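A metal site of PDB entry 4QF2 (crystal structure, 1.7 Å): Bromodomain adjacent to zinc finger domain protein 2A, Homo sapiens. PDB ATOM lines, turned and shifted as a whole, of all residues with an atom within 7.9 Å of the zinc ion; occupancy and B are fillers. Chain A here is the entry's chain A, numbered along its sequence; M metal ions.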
ATOM      1  N   THR A   8      -4.361  22.555 -26.427  1.00  0.00           N
ATOM      2  CA  THR A   8      -5.361  23.586 -26.713  1.00  0.00           C
ATOM      3  C   THR A   8      -6.299  23.132 -27.826  1.00  0.00           C
ATOM      4  O   THR A   8      -5.977  22.289 -28.661  1.00  0.00           O
ATOM      5  CB  THR A   8      -4.730  24.948 -27.057  1.00  0.00           C
ATOM      6  OG1 THR A   8      -3.947  24.811 -28.254  1.00  0.00           O
ATOM      7  CG2 THR A   8      -3.845  25.455 -25.918  1.00  0.00           C
ATOM      8  N   CYS A   9      -7.497  23.682 -27.814  1.00  0.00           N
ATOM      9  CA  CYS A   9      -8.493  23.310 -28.820  1.00  0.00           C
ATOM     10  C   CYS A   9      -8.162  23.956 -30.164  1.00  0.00           C
ATOM     11  O   CYS A   9      -7.897  25.166 -30.257  1.00  0.00           O
ATOM     12  CB  CYS A   9      -9.890  23.777 -28.341  1.00  0.00           C
ATOM     13  SG  CYS A   9     -11.272  23.588 -29.503  1.00  0.00           S
ATOM     14  N   LEU A  10      -8.218  23.155 -31.215  1.00  0.00           N
ATOM     15  CA  LEU A  10      -7.982  23.656 -32.578  1.00  0.00           C
ATOM     16  C   LEU A  10      -8.957  24.722 -33.067  1.00  0.00           C
ATOM     17  O   LEU A  10      -8.576  25.567 -33.866  1.00  0.00           O
ATOM     18  CB  LEU A  10      -7.990  22.514 -33.586  1.00  0.00           C
ATOM     19  CG  LEU A  10      -6.774  21.630 -33.663  1.00  0.00           C
ATOM     20  CD1 LEU A  10      -7.088  20.441 -34.575  1.00  0.00           C
ATOM     21  CD2 LEU A  10      -5.561  22.393 -34.179  1.00  0.00           C
ATOM     22  N   VAL A  11     -10.198  24.653 -32.620  1.00  0.00           N
ATOM     23  CA  VAL A  11     -11.222  25.585 -33.015  1.00  0.00           C
ATOM     24  C   VAL A  11     -11.109  26.921 -32.271  1.00  0.00           C
ATOM     25  O   VAL A  11     -10.969  27.973 -32.908  1.00  0.00           O
ATOM     26  CB  VAL A  11     -12.620  24.933 -32.811  1.00  0.00           C
ATOM     27  CG1 VAL A  11     -13.741  25.885 -33.189  1.00  0.00           C
ATOM     28  CG2 VAL A  11     -12.676  23.635 -33.621  1.00  0.00           C
ATOM     29  N   CYS A  12     -11.194  26.891 -30.951  1.00  0.00           N
ATOM     30  CA  CYS A  12     -11.318  28.115 -30.140  1.00  0.00           C
ATOM     31  C   CYS A  12      -9.980  28.560 -29.545  1.00  0.00           C
ATOM     32  O   CYS A  12      -9.917  29.630 -28.920  1.00  0.00           O
ATOM     33  CB  CYS A  12     -12.316  27.939 -28.994  1.00  0.00           C
ATOM     34  SG  CYS A  12     -11.800  26.821 -27.693  1.00  0.00           S
ATOM     35  N   ARG A  13      -8.965  27.713 -29.678  1.00  0.00           N
ATOM     36  CA  ARG A  13      -7.582  28.003 -29.201  1.00  0.00           C
ATOM     37  C   ARG A  13      -7.405  28.074 -27.677  1.00  0.00           C
ATOM     38  O   ARG A  13      -6.339  28.479 -27.209  1.00  0.00           O
ATOM     39  CB  ARG A  13      -7.056  29.304 -29.815  1.00  0.00           C
ATOM     40  CG  ARG A  13      -7.282  29.475 -31.301  1.00  0.00           C
ATOM     41  CD  ARG A  13      -6.530  28.449 -32.123  1.00  0.00           C
ATOM     42  NE  ARG A  13      -6.198  28.962 -33.444  1.00  0.00           N
ATOM     43  CZ  ARG A  13      -5.612  28.256 -34.416  1.00  0.00           C
ATOM     44  NH1 ARG A  13      -5.299  26.977 -34.226  1.00  0.00           N
ATOM     45  NH2 ARG A  13      -5.353  28.834 -35.586  1.00  0.00           N
ATOM     46  N   LYS A  14      -8.419  27.736 -26.912  1.00  0.00           N
ATOM     47  CA  LYS A  14      -8.322  27.703 -25.454  1.00  0.00           C
ATOM     48  C   LYS A  14      -8.005  26.281 -24.965  1.00  0.00           C
ATOM     49  O   LYS A  14      -8.330  25.276 -25.606  1.00  0.00           O
ATOM     50  CB  LYS A  14      -9.604  28.169 -24.783  1.00  0.00           C
ATOM     51  CG  LYS A  14     -10.179  29.490 -25.272  1.00  0.00           C
ATOM     52  CD  LYS A  14     -10.999  30.140 -24.157  1.00  0.00           C
ATOM     53  CE  LYS A  14     -12.438  30.444 -24.545  1.00  0.00           C
ATOM     54  NZ  LYS A  14     -12.555  31.552 -25.525  1.00  0.00           N
ATOM     55  N   GLY A  15      -7.366  26.196 -23.804  1.00  0.00           N
ATOM     56  CA  GLY A  15      -7.091  24.909 -23.176  1.00  0.00           C
ATOM     57  C   GLY A  15      -7.880  24.667 -21.902  1.00  0.00           C
ATOM     58  O   GLY A  15      -7.481  23.837 -21.085  1.00  0.00           O
ATOM     59  N   ASP A  16      -8.989  25.402 -21.720  1.00  0.00           N
ATOM     60  CA  ASP A  16      -9.821  25.239 -20.516  1.00  0.00           C
ATOM     61  C   ASP A  16     -10.767  24.050 -20.669  1.00  0.00           C
ATOM     62  O   ASP A  16     -10.837  23.442 -21.725  1.00  0.00           O
ATOM     63  CB  ASP A  16     -10.591  26.522 -20.155  1.00  0.00           C
ATOM     64  CG  ASP A  16     -11.478  27.044 -21.297  1.00  0.00           C
ATOM     65  OD1 ASP A  16     -11.512  26.443 -22.381  1.00  0.00           O
ATOM     66  OD2 ASP A  16     -12.143  28.090 -21.109  1.00  0.00           O
ATOM     67  N   PHE A  20     -13.458  18.116 -21.274  1.00  0.00           N
ATOM     68  CA  PHE A  20     -14.200  18.142 -22.552  1.00  0.00           C
ATOM     69  C   PHE A  20     -13.316  18.131 -23.791  1.00  0.00           C
ATOM     70  O   PHE A  20     -13.788  18.185 -24.931  1.00  0.00           O
ATOM     71  CB  PHE A  20     -15.086  19.382 -22.614  1.00  0.00           C
ATOM     72  CG  PHE A  20     -16.216  19.366 -21.652  1.00  0.00           C
ATOM     73  CD1 PHE A  20     -16.039  19.802 -20.346  1.00  0.00           C
ATOM     74  CD2 PHE A  20     -17.452  18.913 -22.030  1.00  0.00           C
ATOM     75  CE1 PHE A  20     -17.086  19.792 -19.451  1.00  0.00           C
ATOM     76  CE2 PHE A  20     -18.522  18.903 -21.131  1.00  0.00           C
ATOM     77  CZ  PHE A  20     -18.328  19.337 -19.859  1.00  0.00           C
ATOM     78  N   LEU A  21     -12.013  18.051 -23.571  1.00  0.00           N
ATOM     79  CA  LEU A  21     -11.028  18.121 -24.653  1.00  0.00           C
ATOM     80  C   LEU A  21     -10.739  16.731 -25.246  1.00  0.00           C
ATOM     81  O   LEU A  21     -10.215  15.861 -24.553  1.00  0.00           O
ATOM     82  CB  LEU A  21      -9.771  18.782 -24.063  1.00  0.00           C
ATOM     83  CG  LEU A  21      -8.807  19.671 -24.797  1.00  0.00           C
ATOM     84  CD1 LEU A  21      -9.455  20.550 -25.845  1.00  0.00           C
ATOM     85  CD2 LEU A  21      -8.088  20.531 -23.750  1.00  0.00           C
ATOM     86  N   GLY A  30      -5.729  19.022 -30.107  1.00  0.00           N
ATOM     87  CA  GLY A  30      -6.974  18.719 -29.381  1.00  0.00           C
ATOM     88  C   GLY A  30      -8.165  19.472 -29.881  1.00  0.00           C
ATOM     89  O   GLY A  30      -8.052  20.346 -30.742  1.00  0.00           O
ATOM     90  N   CYS A  31      -9.342  19.124 -29.339  1.00  0.00           N
ATOM     91  CA  CYS A  31     -10.583  19.831 -29.711  1.00  0.00           C
ATOM     92  C   CYS A  31     -11.618  19.638 -28.608  1.00  0.00           C
ATOM     93  O   CYS A  31     -11.865  18.536 -28.231  1.00  0.00           O
ATOM     94  CB  CYS A  31     -11.165  19.269 -31.018  1.00  0.00           C
ATOM     95  SG  CYS A  31     -12.548  20.208 -31.711  1.00  0.00           S
ATOM     96  N   HIS A  32     -12.232  20.730 -28.116  1.00  0.00           N
ATOM     97  CA  HIS A  32     -13.358  20.572 -27.182  1.00  0.00           C
ATOM     98  C   HIS A  32     -14.487  19.827 -27.923  1.00  0.00           C
ATOM     99  O   HIS A  32     -14.838  20.149 -29.071  1.00  0.00           O
ATOM    100  CB  HIS A  32     -13.928  21.928 -26.694  1.00  0.00           C
ATOM    101  CG  HIS A  32     -12.980  22.708 -25.838  1.00  0.00           C
ATOM    102  ND1 HIS A  32     -12.432  23.908 -26.232  1.00  0.00           N
ATOM    103  CD2 HIS A  32     -12.504  22.456 -24.599  1.00  0.00           C
ATOM    104  CE1 HIS A  32     -11.657  24.363 -25.271  1.00  0.00           C
ATOM    105  NE2 HIS A  32     -11.662  23.496 -24.279  1.00  0.00           N
ATOM    106  N   ILE A  33     -15.144  18.906 -27.247  1.00  0.00           N
ATOM    107  CA  ILE A  33     -16.326  18.291 -27.857  1.00  0.00           C
ATOM    108  C   ILE A  33     -17.391  19.303 -28.262  1.00  0.00           C
ATOM    109  O   ILE A  33     -18.033  19.155 -29.287  1.00  0.00           O
ATOM    110  CB  ILE A  33     -16.936  17.160 -27.027  1.00  0.00           C
ATOM    111  CG1 ILE A  33     -17.353  17.625 -25.636  1.00  0.00           C
ATOM    112  CG2 ILE A  33     -15.960  16.018 -26.868  1.00  0.00           C
ATOM    113  CD1 ILE A  33     -18.237  16.564 -25.004  1.00  0.00           C
ATOM    114  N   TYR A  34     -17.525  20.379 -27.506  1.00  0.00           N
ATOM    115  CA  TYR A  34     -18.550  21.376 -27.774  1.00  0.00           C
ATOM    116  C   TYR A  34     -18.193  22.310 -28.914  1.00  0.00           C
ATOM    117  O   TYR A  34     -19.072  22.967 -29.435  1.00  0.00           O
ATOM    118  CB  TYR A  34     -18.840  22.167 -26.489  1.00  0.00           C
ATOM    119  CG  TYR A  34     -17.668  22.688 -25.726  1.00  0.00           C
ATOM    120  CD1 TYR A  34     -17.062  23.894 -26.102  1.00  0.00           C
ATOM    121  CD2 TYR A  34     -17.249  22.111 -24.517  1.00  0.00           C
ATOM    122  CE1 TYR A  34     -16.059  24.468 -25.330  1.00  0.00           C
ATOM    123  CE2 TYR A  34     -16.277  22.703 -23.741  1.00  0.00           C
ATOM    124  CZ  TYR A  34     -15.672  23.865 -24.163  1.00  0.00           C
ATOM    125  OH  TYR A  34     -14.652  24.447 -23.396  1.00  0.00           O
ATOM    126  N   CYS A  35     -16.926  22.313 -29.339  1.00  0.00           N
ATOM    127  CA  CYS A  35     -16.472  23.083 -30.494  1.00  0.00           C
ATOM    128  C   CYS A  35     -16.527  22.273 -31.790  1.00  0.00           C
ATOM    129  O   CYS A  35     -16.539  22.877 -32.857  1.00  0.00           O
ATOM    130  CB  CYS A  35     -15.043  23.506 -30.315  1.00  0.00           C
ATOM    131  SG  CYS A  35     -14.867  24.771 -28.983  1.00  0.00           S
ATOM    132  N   HIS A  36     -16.605  20.952 -31.662  1.00  0.00           N
ATOM    133  CA  HIS A  36     -16.640  20.074 -32.822  1.00  0.00           C
ATOM    134  C   HIS A  36     -17.955  20.237 -33.580  1.00  0.00           C
ATOM    135  O   HIS A  36     -19.036  20.421 -33.004  1.00  0.00           O
ATOM    136  CB  HIS A  36     -16.445  18.650 -32.370  1.00  0.00           C
ATOM    137  CG  HIS A  36     -16.023  17.711 -33.452  1.00  0.00           C
ATOM    138  ND1 HIS A  36     -16.918  17.210 -34.385  1.00  0.00           N
ATOM    139  CD2 HIS A  36     -14.824  17.184 -33.743  1.00  0.00           C
ATOM    140  CE1 HIS A  36     -16.269  16.401 -35.206  1.00  0.00           C
ATOM    141  NE2 HIS A  36     -15.009  16.345 -34.837  1.00  0.00           N
HETATM  142 ZN    ZN M   1     -12.724  24.790 -28.140  1.00  0.00          ZN
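NE2 of His 32 lies within hydrogen-bond range of O of Asp 16 (2.7 Å). The backbone NH (N) of Lys 14 sits close to the side-chain sulfur (SG) of Cys 12 (3.6 Å). The backbone NH of Cys 9 sits at hydrogen-bond distance from the backbone carbonyl oxygen of Lys 14. A ring nitrogen (NE2) of His 32 lies close to the side-chain hydroxyl (OH) of Tyr 34 (3.3 Å). SG of Cys 9 sits close to N of Val 11.
Within 4 Å of the zinc ion: Cys 9, Cys 12, His 32 and Cys 35. The nearest printed residue that does not touch the zinc ion is Tyr 34 (4.4 Å).
The zinc ion is bound by a ring nitrogen (ND1) of His 32, the side-chain sulfur of Cys 12, the side-chain sulfur of Cys 35 and the side-chain sulfur of Cys 9. The zinc ion has four donor atoms within binding distance.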
